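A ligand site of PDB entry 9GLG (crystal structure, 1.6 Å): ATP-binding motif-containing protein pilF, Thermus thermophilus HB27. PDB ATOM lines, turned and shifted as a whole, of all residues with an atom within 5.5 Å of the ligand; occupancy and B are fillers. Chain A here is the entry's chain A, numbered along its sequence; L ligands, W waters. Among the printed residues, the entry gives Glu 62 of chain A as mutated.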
ATOM      1  N   LEU A  10     -12.911  -8.133  10.660  1.00  0.00           N
ATOM      2  CA  LEU A  10     -13.304  -7.798  12.019  1.00  0.00           C
ATOM      3  C   LEU A  10     -12.223  -8.222  13.004  1.00  0.00           C
ATOM      4  O   LEU A  10     -11.584  -9.267  12.836  1.00  0.00           O
ATOM      5  CB  LEU A  10     -14.633  -8.470  12.383  1.00  0.00           C
ATOM      6  CG  LEU A  10     -15.895  -7.946  11.690  1.00  0.00           C
ATOM      7  CD1 LEU A  10     -17.142  -8.482  12.383  1.00  0.00           C
ATOM      8  CD2 LEU A  10     -15.924  -6.425  11.660  1.00  0.00           C
ATOM      9  N   LYS A  11     -12.008  -7.393  14.016  1.00  0.00           N
ATOM     10  CA  LYS A  11     -11.146  -7.769  15.136  1.00  0.00           C
ATOM     11  C   LYS A  11     -11.936  -8.606  16.140  1.00  0.00           C
ATOM     12  O   LYS A  11     -13.162  -8.760  16.032  1.00  0.00           O
ATOM     13  CB  LYS A  11     -10.564  -6.525  15.799  1.00  0.00           C
ATOM     14  CG  LYS A  11      -9.717  -5.667  14.860  1.00  0.00           C
ATOM     15  CD  LYS A  11      -9.238  -4.405  15.551  1.00  0.00           C
ATOM     16  CE  LYS A  11      -8.579  -3.442  14.578  1.00  0.00           C
ATOM     17  NZ  LYS A  11      -7.383  -4.055  13.929  1.00  0.00           N
ATOM     18  N   LEU A  12     -11.226  -9.141  17.137  1.00  0.00           N
ATOM     19  CA  LEU A  12     -11.828 -10.066  18.091  1.00  0.00           C
ATOM     20  C   LEU A  12     -13.040  -9.458  18.788  1.00  0.00           C
ATOM     21  O   LEU A  12     -14.077 -10.121  18.931  1.00  0.00           O
ATOM     22  CB  LEU A  12     -10.799 -10.489  19.128  1.00  0.00           C
ATOM     23  CG  LEU A  12     -11.357 -11.274  20.305  1.00  0.00           C
ATOM     24  CD1 LEU A  12     -11.937 -12.627  19.871  1.00  0.00           C
ATOM     25  CD2 LEU A  12     -10.293 -11.465  21.360  1.00  0.00           C
ATOM     26  N   GLY A  13     -12.895  -8.233  19.299  1.00  0.00           N
ATOM     27  CA  GLY A  13     -14.001  -7.644  20.042  1.00  0.00           C
ATOM     28  C   GLY A  13     -15.226  -7.444  19.173  1.00  0.00           C
ATOM     29  O   GLY A  13     -16.347  -7.765  19.584  1.00  0.00           O
ATOM     30  N   GLU A  14     -15.012  -6.968  17.946  1.00  0.00           N
ATOM     31  CA  GLU A  14     -16.113  -6.759  17.012  1.00  0.00           C
ATOM     32  C   GLU A  14     -16.827  -8.059  16.702  1.00  0.00           C
ATOM     33  O   GLU A  14     -18.059  -8.097  16.602  1.00  0.00           O
ATOM     34  CB  GLU A  14     -15.583  -6.118  15.721  1.00  0.00           C
ATOM     35  CG  GLU A  14     -15.158  -4.656  15.886  1.00  0.00           C
ATOM     36  CD  GLU A  14     -14.242  -4.142  14.769  1.00  0.00           C
ATOM     37  OE1 GLU A  14     -13.451  -4.938  14.205  1.00  0.00           O
ATOM     38  OE2 GLU A  14     -14.320  -2.938  14.455  1.00  0.00           O
ATOM     39  N   LEU A  27     -16.923  -4.749  26.283  1.00  0.00           N
ATOM     40  CA  LEU A  27     -15.804  -4.581  25.345  1.00  0.00           C
ATOM     41  C   LEU A  27     -15.031  -3.311  25.653  1.00  0.00           C
ATOM     42  O   LEU A  27     -13.800  -3.326  25.741  1.00  0.00           O
ATOM     43  CB  LEU A  27     -16.313  -4.560  23.912  1.00  0.00           C
ATOM     44  CG  LEU A  27     -15.268  -4.303  22.812  1.00  0.00           C
ATOM     45  CD1 LEU A  27     -14.089  -5.288  22.920  1.00  0.00           C
ATOM     46  CD2 LEU A  27     -15.900  -4.367  21.442  1.00  0.00           C
ATOM     47  N   LEU A  31     -11.045  -2.950  26.668  1.00  0.00           N
ATOM     48  CA  LEU A  31     -10.105  -2.150  25.885  1.00  0.00           C
ATOM     49  C   LEU A  31      -9.471  -1.052  26.736  1.00  0.00           C
ATOM     50  O   LEU A  31      -8.278  -0.736  26.564  1.00  0.00           O
ATOM     51  CB  LEU A  31     -10.799  -1.542  24.662  1.00  0.00           C
ATOM     52  CG  LEU A  31     -11.183  -2.521  23.556  1.00  0.00           C
ATOM     53  CD1 LEU A  31     -12.125  -1.862  22.562  1.00  0.00           C
ATOM     54  CD2 LEU A  31      -9.955  -3.076  22.845  1.00  0.00           C
ATOM     55  N   GLN A  34      -6.812  -2.754  28.726  1.00  0.00           N
ATOM     56  CA  GLN A  34      -5.689  -3.094  27.870  1.00  0.00           C
ATOM     57  C   GLN A  34      -4.813  -1.877  27.586  1.00  0.00           C
ATOM     58  O   GLN A  34      -3.582  -1.987  27.542  1.00  0.00           O
ATOM     59  CB  GLN A  34      -6.185  -3.695  26.555  1.00  0.00           C
ATOM     60  CG  GLN A  34      -5.049  -4.047  25.620  1.00  0.00           C
ATOM     61  CD  GLN A  34      -5.547  -4.652  24.327  1.00  0.00           C
ATOM     62  OE1 GLN A  34      -6.143  -3.961  23.508  1.00  0.00           O
ATOM     63  NE2 GLN A  34      -5.268  -5.938  24.128  1.00  0.00           N
ATOM     64  N   GLY A  38      -1.634  -3.598  28.558  1.00  0.00           N
ATOM     65  CA  GLY A  38      -1.062  -4.325  27.448  1.00  0.00           C
ATOM     66  C   GLY A  38      -1.362  -5.805  27.418  1.00  0.00           C
ATOM     67  O   GLY A  38      -0.820  -6.514  26.554  1.00  0.00           O
ATOM     68  N   ASP A  39      -2.205  -6.313  28.317  1.00  0.00           N
ATOM     69  CA  ASP A  39      -2.604  -7.712  28.283  1.00  0.00           C
ATOM     70  C   ASP A  39      -3.373  -8.013  26.994  1.00  0.00           C
ATOM     71  O   ASP A  39      -3.970  -7.130  26.375  1.00  0.00           O
ATOM     72  CB  ASP A  39      -3.482  -8.074  29.488  1.00  0.00           C
ATOM     73  CG  ASP A  39      -2.661  -8.424  30.731  1.00  0.00           C
ATOM     74  OD1 ASP A  39      -1.421  -8.280  30.694  1.00  0.00           O
ATOM     75  OD2 ASP A  39      -3.269  -8.835  31.741  1.00  0.00           O
ATOM     76  N   LEU A  40      -3.350  -9.290  26.601  1.00  0.00           N
ATOM     77  CA  LEU A  40      -4.139  -9.759  25.461  1.00  0.00           C
ATOM     78  C   LEU A  40      -5.616  -9.525  25.706  1.00  0.00           C
ATOM     79  O   LEU A  40      -6.120  -9.778  26.802  1.00  0.00           O
ATOM     80  CB  LEU A  40      -3.930 -11.256  25.236  1.00  0.00           C
ATOM     81  CG  LEU A  40      -2.977 -11.815  24.188  1.00  0.00           C
ATOM     82  CD1 LEU A  40      -3.141 -13.330  24.171  1.00  0.00           C
ATOM     83  CD2 LEU A  40      -3.220 -11.200  22.802  1.00  0.00           C
ATOM     84  N   LEU A  41      -6.327  -9.069  24.662  1.00  0.00           N
ATOM     85  CA  LEU A  41      -7.728  -8.685  24.864  1.00  0.00           C
ATOM     86  C   LEU A  41      -8.573  -9.877  25.309  1.00  0.00           C
ATOM     87  O   LEU A  41      -9.362  -9.766  26.247  1.00  0.00           O
ATOM     88  CB  LEU A  41      -8.317  -8.091  23.592  1.00  0.00           C
ATOM     89  CG  LEU A  41      -9.717  -7.493  23.824  1.00  0.00           C
ATOM     90  CD1 LEU A  41      -9.634  -6.311  24.771  1.00  0.00           C
ATOM     91  CD2 LEU A  41     -10.395  -7.104  22.511  1.00  0.00           C
ATOM     92  N   GLY A  42      -8.416 -11.024  24.639  1.00  0.00           N
ATOM     93  CA  GLY A  42      -9.193 -12.185  25.018  1.00  0.00           C
ATOM     94  C   GLY A  42      -8.972 -12.599  26.453  1.00  0.00           C
ATOM     95  O   GLY A  42      -9.917 -12.981  27.160  1.00  0.00           O
ATOM     96  N   ARG A  43      -7.731 -12.499  26.935  1.00  0.00           N
ATOM     97  CA  ARG A  43      -7.437 -12.831  28.326  1.00  0.00           C
ATOM     98  C   ARG A  43      -8.180 -11.903  29.282  1.00  0.00           C
ATOM     99  O   ARG A  43      -8.706 -12.351  30.314  1.00  0.00           O
ATOM    100  CB  ARG A  43      -5.933 -12.788  28.583  1.00  0.00           C
ATOM    101  CG  ARG A  43      -5.292 -14.161  28.474  1.00  0.00           C
ATOM    102  CD  ARG A  43      -3.980 -14.242  29.253  1.00  0.00           C
ATOM    103  NE  ARG A  43      -2.855 -13.663  28.533  1.00  0.00           N
ATOM    104  CZ  ARG A  43      -2.296 -14.202  27.446  1.00  0.00           C
ATOM    105  NH1 ARG A  43      -2.757 -15.340  26.946  1.00  0.00           N
ATOM    106  NH2 ARG A  43      -1.266 -13.590  26.867  1.00  0.00           N
ATOM    107  N   LEU A  55     -14.421 -17.323  23.564  1.00  0.00           N
ATOM    108  CA  LEU A  55     -13.222 -16.703  23.020  1.00  0.00           C
ATOM    109  C   LEU A  55     -12.627 -17.552  21.908  1.00  0.00           C
ATOM    110  O   LEU A  55     -12.296 -17.044  20.831  1.00  0.00           O
ATOM    111  CB  LEU A  55     -12.197 -16.482  24.129  1.00  0.00           C
ATOM    112  CG  LEU A  55     -10.795 -16.102  23.672  1.00  0.00           C
ATOM    113  CD1 LEU A  55     -10.834 -14.726  23.000  1.00  0.00           C
ATOM    114  CD2 LEU A  55      -9.817 -16.123  24.850  1.00  0.00           C
ATOM    115  N   TYR A  56     -12.500 -18.863  22.146  1.00  0.00           N
ATOM    116  CA  TYR A  56     -11.791 -19.681  21.174  1.00  0.00           C
ATOM    117  C   TYR A  56     -12.614 -19.877  19.909  1.00  0.00           C
ATOM    118  O   TYR A  56     -12.058 -19.953  18.812  1.00  0.00           O
ATOM    119  CB  TYR A  56     -11.403 -21.024  21.796  1.00  0.00           C
ATOM    120  CG  TYR A  56     -10.061 -20.965  22.485  1.00  0.00           C
ATOM    121  CD1 TYR A  56      -9.880 -20.210  23.633  1.00  0.00           C
ATOM    122  CD2 TYR A  56      -8.962 -21.630  21.954  1.00  0.00           C
ATOM    123  CE1 TYR A  56      -8.642 -20.127  24.255  1.00  0.00           C
ATOM    124  CE2 TYR A  56      -7.717 -21.565  22.572  1.00  0.00           C
ATOM    125  CZ  TYR A  56      -7.564 -20.799  23.720  1.00  0.00           C
ATOM    126  OH  TYR A  56      -6.335 -20.729  24.333  1.00  0.00           O
ATOM    127  N   LEU A  59     -11.962 -16.683  18.057  1.00  0.00           N
ATOM    128  CA  LEU A  59     -10.601 -16.675  17.503  1.00  0.00           C
ATOM    129  C   LEU A  59     -10.494 -17.623  16.317  1.00  0.00           C
ATOM    130  O   LEU A  59      -9.787 -17.330  15.330  1.00  0.00           O
ATOM    131  CB  LEU A  59      -9.593 -17.049  18.581  1.00  0.00           C
ATOM    132  CG  LEU A  59      -9.336 -16.037  19.702  1.00  0.00           C
ATOM    133  CD1 LEU A  59      -8.487 -16.698  20.793  1.00  0.00           C
ATOM    134  CD2 LEU A  59      -8.671 -14.786  19.186  1.00  0.00           C
ATOM    135  N   GLU A  62     -12.085 -15.911  13.358  1.00  0.00           N
ATOM    136  CA  GLU A  62     -11.252 -14.799  12.903  1.00  0.00           C
ATOM    137  C   GLU A  62     -10.112 -15.278  12.004  1.00  0.00           C
ATOM    138  O   GLU A  62      -9.751 -14.613  11.030  1.00  0.00           O
ATOM    139  CB  GLU A  62     -10.695 -14.056  14.118  1.00  0.00           C
ATOM    140  CG  GLU A  62      -9.799 -12.870  13.814  1.00  0.00           C
ATOM    141  CD  GLU A  62      -9.432 -12.100  15.055  1.00  0.00           C
ATOM    142  OE1 GLU A  62      -9.589 -10.869  15.058  1.00  0.00           O
ATOM    143  OE2 GLU A  62      -8.996 -12.725  16.041  1.00  0.00           O
ATOM    144  N   LYS A  63      -9.552 -16.447  12.316  1.00  0.00           N
ATOM    145  CA  LYS A  63      -8.364 -16.947  11.632  1.00  0.00           C
ATOM    146  C   LYS A  63      -8.662 -18.040  10.618  1.00  0.00           C
ATOM    147  O   LYS A  63      -7.718 -18.661  10.102  1.00  0.00           O
ATOM    148  CB  LYS A  63      -7.342 -17.436  12.657  1.00  0.00           C
ATOM    149  CG  LYS A  63      -6.613 -16.322  13.400  1.00  0.00           C
ATOM    150  CD  LYS A  63      -5.770 -15.486  12.451  1.00  0.00           C
ATOM    151  CE  LYS A  63      -4.716 -16.332  11.738  1.00  0.00           C
ATOM    152  NZ  LYS A  63      -3.906 -15.546  10.756  1.00  0.00           N
ATOM    153  N   SER A 109      -3.050 -24.939  19.256  1.00  0.00           N
ATOM    154  CA  SER A 109      -3.461 -24.458  20.563  1.00  0.00           C
ATOM    155  C   SER A 109      -3.714 -22.954  20.602  1.00  0.00           C
ATOM    156  O   SER A 109      -4.390 -22.464  21.516  1.00  0.00           O
ATOM    157  CB  SER A 109      -2.384 -24.807  21.607  1.00  0.00           C
ATOM    158  OG  SER A 109      -1.221 -24.014  21.402  1.00  0.00           O
ATOM    159  N   ASP A 110      -3.158 -22.224  19.646  1.00  0.00           N
ATOM    160  CA  ASP A 110      -3.165 -20.768  19.658  1.00  0.00           C
ATOM    161  C   ASP A 110      -3.343 -20.333  18.209  1.00  0.00           C
ATOM    162  O   ASP A 110      -2.481 -20.621  17.375  1.00  0.00           O
ATOM    163  CB  ASP A 110      -1.857 -20.244  20.252  1.00  0.00           C
ATOM    164  CG  ASP A 110      -1.870 -18.736  20.491  1.00  0.00           C
ATOM    165  OD1 ASP A 110      -2.609 -18.018  19.799  1.00  0.00           O
ATOM    166  OD2 ASP A 110      -1.112 -18.285  21.376  1.00  0.00           O
ATOM    167  N   PRO A 111      -4.443 -19.656  17.868  1.00  0.00           N
ATOM    168  CA  PRO A 111      -4.629 -19.213  16.476  1.00  0.00           C
ATOM    169  C   PRO A 111      -3.513 -18.308  15.985  1.00  0.00           C
ATOM    170  O   PRO A 111      -3.283 -18.222  14.767  1.00  0.00           O
ATOM    171  CB  PRO A 111      -5.966 -18.466  16.522  1.00  0.00           C
ATOM    172  CG  PRO A 111      -6.074 -17.989  17.932  1.00  0.00           C
ATOM    173  CD  PRO A 111      -5.495 -19.105  18.750  1.00  0.00           C
ATOM    174  N   ARG A 112      -2.809 -17.609  16.889  1.00  0.00           N
ATOM    175  CA  ARG A 112      -1.747 -16.698  16.482  1.00  0.00           C
ATOM    176  C   ARG A 112      -0.564 -17.432  15.864  1.00  0.00           C
ATOM    177  O   ARG A 112       0.264 -16.790  15.211  1.00  0.00           O
ATOM    178  CB  ARG A 112      -1.271 -15.883  17.664  1.00  0.00           C
ATOM    179  CG  ARG A 112      -2.307 -14.913  18.228  1.00  0.00           C
ATOM    180  CD  ARG A 112      -1.783 -14.208  19.463  1.00  0.00           C
ATOM    181  NE  ARG A 112      -1.548 -15.174  20.539  1.00  0.00           N
ATOM    182  CZ  ARG A 112      -0.961 -14.879  21.691  1.00  0.00           C
ATOM    183  NH1 ARG A 112      -0.791 -15.819  22.611  1.00  0.00           N
ATOM    184  NH2 ARG A 112      -0.517 -13.653  21.924  1.00  0.00           N
HETATM  185  P1  LIG L   1      -7.078  -8.900  16.483  1.00  0.00           P
HETATM  186  O1  LIG L   1      -8.414  -9.495  16.832  1.00  0.00           O
HETATM  187  O2  LIG L   1      -7.108  -8.544  15.020  1.00  0.00           O
HETATM  188  O3  LIG L   1      -6.840  -7.535  17.328  1.00  0.00           O
HETATM  189  C1  LIG L   1      -5.601  -6.817  17.104  1.00  0.00           C
HETATM  190  C2  LIG L   1      -5.580  -5.754  18.249  1.00  0.00           C
HETATM  191  O4  LIG L   1      -6.660  -5.051  18.104  1.00  0.00           O
HETATM  192  C3  LIG L   1      -5.722  -6.488  19.598  1.00  0.00           C
HETATM  193  O5  LIG L   1      -4.472  -6.612  20.068  1.00  0.00           O
HETATM  194  C4  LIG L   1      -6.592  -5.529  20.463  1.00  0.00           C
HETATM  195  O6  LIG L   1      -5.672  -4.544  21.142  1.00  0.00           O
HETATM  196  C5  LIG L   1      -7.263  -4.838  19.597  1.00  0.00           C
HETATM  197  N1  LIG L   1      -8.702  -4.887  19.453  1.00  0.00           N
HETATM  198  C6  LIG L   1      -9.037  -6.221  19.389  1.00  0.00           C
HETATM  199  N2  LIG L   1     -10.410  -6.282  19.222  1.00  0.00           N
HETATM  200  C7  LIG L   1     -10.879  -5.011  19.147  1.00  0.00           C
HETATM  201  C8  LIG L   1     -12.244  -4.320  18.967  1.00  0.00           C
HETATM  202  O7  LIG L   1     -13.260  -4.910  18.829  1.00  0.00           O
HETATM  203  N3  LIG L   1     -12.319  -2.896  18.938  1.00  0.00           N
HETATM  204  C9  LIG L   1     -11.139  -2.085  19.080  1.00  0.00           C
HETATM  205  N4  LIG L   1     -11.206  -0.648  19.059  1.00  0.00           N
HETATM  206  N5  LIG L   1      -9.866  -2.736  19.253  1.00  0.00           N
HETATM  207  C10 LIG L   1      -9.805  -4.200  19.285  1.00  0.00           C
HETATM  208  P2  LIG L   1      -4.249  -7.910  21.187  1.00  0.00           P
HETATM  209  O8  LIG L   1      -5.230  -7.867  22.351  1.00  0.00           O
HETATM  210  O9  LIG L   1      -2.815  -7.913  21.649  1.00  0.00           O
HETATM  211  O10 LIG L   1      -4.567  -9.289  20.189  1.00  0.00           O
HETATM  212  C11 LIG L   1      -3.608  -9.612  19.181  1.00  0.00           C
HETATM  213  C12 LIG L   1      -4.143 -10.826  18.460  1.00  0.00           C
HETATM  214  O11 LIG L   1      -4.095 -11.886  19.226  1.00  0.00           O
HETATM  215  C13 LIG L   1      -5.761 -10.667  18.049  1.00  0.00           C
HETATM  216  O12 LIG L   1      -5.815 -10.038  16.659  1.00  0.00           O
HETATM  217  C14 LIG L   1      -6.253 -11.807  18.071  1.00  0.00           C
HETATM  218  O13 LIG L   1      -6.005 -12.567  16.779  1.00  0.00           O
HETATM  219  C15 LIG L   1      -5.425 -12.593  19.196  1.00  0.00           C
HETATM  220  N6  LIG L   1      -5.948 -12.540  20.429  1.00  0.00           N
HETATM  221  C16 LIG L   1      -6.583 -11.562  21.126  1.00  0.00           C
HETATM  222  N7  LIG L   1      -6.829 -12.086  22.362  1.00  0.00           N
HETATM  223  C17 LIG L   1      -6.341 -13.326  22.431  1.00  0.00           C
HETATM  224  C18 LIG L   1      -6.318 -14.368  23.559  1.00  0.00           C
HETATM  225  O14 LIG L   1      -6.783 -14.169  24.618  1.00  0.00           O
HETATM  226  N8  LIG L   1      -5.710 -15.629  23.306  1.00  0.00           N
HETATM  227  C19 LIG L   1      -5.125 -15.899  22.020  1.00  0.00           C
HETATM  228  N9  LIG L   1      -4.496 -17.220  21.779  1.00  0.00           N
HETATM  229  N10 LIG L   1      -5.168 -14.921  20.950  1.00  0.00           N
HETATM  230  C20 LIG L   1      -5.778 -13.607  21.205  1.00  0.00           C
HETATM  231  O   HOH W   1      -0.312  -9.243  22.339  1.00  0.00           O
HETATM  232  O   HOH W   2      -7.673  -1.479  17.751  1.00  0.00           O
HETATM  233  O   HOH W   3      -2.853  -3.904  20.824  1.00  0.00           O
HETATM  234  O   HOH W   4      -5.157 -14.627  15.767  1.00  0.00           O
HETATM  235  O   HOH W   5      -3.559 -10.810  14.643  1.00  0.00           O
HETATM  236  O   HOH W   6      -5.083  -7.510  13.462  1.00  0.00           O
HETATM  237  O   HOH W   7      -8.592  -9.247  12.631  1.00  0.00           O
HETATM  238  O   HOH W   8      -0.886  -7.220  19.430  1.00  0.00           O
HETATM  239  O   HOH W   9      -4.144 -20.005  23.032  1.00  0.00           O
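Water W7 lies within hydrogen-bond range of an oxygen (O2) of the ligand, the backbone carbonyl oxygen of Leu 10 and the side-chain carboxylate of Glu 62. Water W9 lies within hydrogen-bond range of the side-chain hydroxyl of Tyr 56, the backbone carbonyl oxygen of Ser 109 and a nitrogen (N9) of the ligand.
Merely in contact with the ligand: Lys 11 (3.4 Å), Leu 27 (3.8 Å), Leu 31 (3.6 Å), Leu 40 (3.4 Å), Leu 55 (3.6 Å), Leu 59 (3.7 Å), Pro 111 (3.7 Å) and Arg 112 (3.3 Å). Within 4 Å of the ligand: Lys 11, Leu 12, Gly 13, Glu 14, Leu 27, Leu 31, Gln 34, Leu 40, Leu 41, Gly 42, Arg 43, Leu 55, Leu 59, Glu 62, Asp 110, Pro 111 and Arg 112.
The backbone NH of Leu 41 sits at hydrogen-bond distance from an oxygen (O8) of the ligand. A nitrogen (N9) of the ligand lies within hydrogen-bond range of the side-chain carboxylate of Asp 110 (2.8 Å). The backbone NH (N) of Gly 42 lies within hydrogen-bond range of a nitrogen (N7) of the ligand, at 3.0 Å. OE2 of Glu 62 lies within hydrogen-bond range of O13 of the ligand (3.1 Å). The side-chain amide oxygen (OE1) of Gln 34 lies within hydrogen-bond range of an oxygen (O6) of the ligand (2.5 Å). N of Glu 14 lies within hydrogen-bond range of O7 of the ligand (2.8 Å). A nitrogen (N2) of the ligand sits at hydrogen-bond distance from the backbone NH (N) of Gly 13 (3.2 Å). N of Arg 43 is in hydrogen-bond range of O14 of the ligand. N of Leu 12 sits at hydrogen-bond distance from O1 of the ligand (2.9 Å).
O of Asp 39 is in hydrogen-bond range of NE2 of Gln 34 (2.9 Å). OE1 of Glu 14 sits at hydrogen-bond distance from N of Lys 11 (2.9 Å). OE1 of Glu 62 lies within hydrogen-bond range of N of Leu 12 (3.2 Å). NE2 of Gln 34 lies close to N of Leu 41 (3.3 Å). The side-chain carboxylate of Asp 110 is in salt-bridge range of the guanidinium group of Arg 112, 2.8 Å away.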
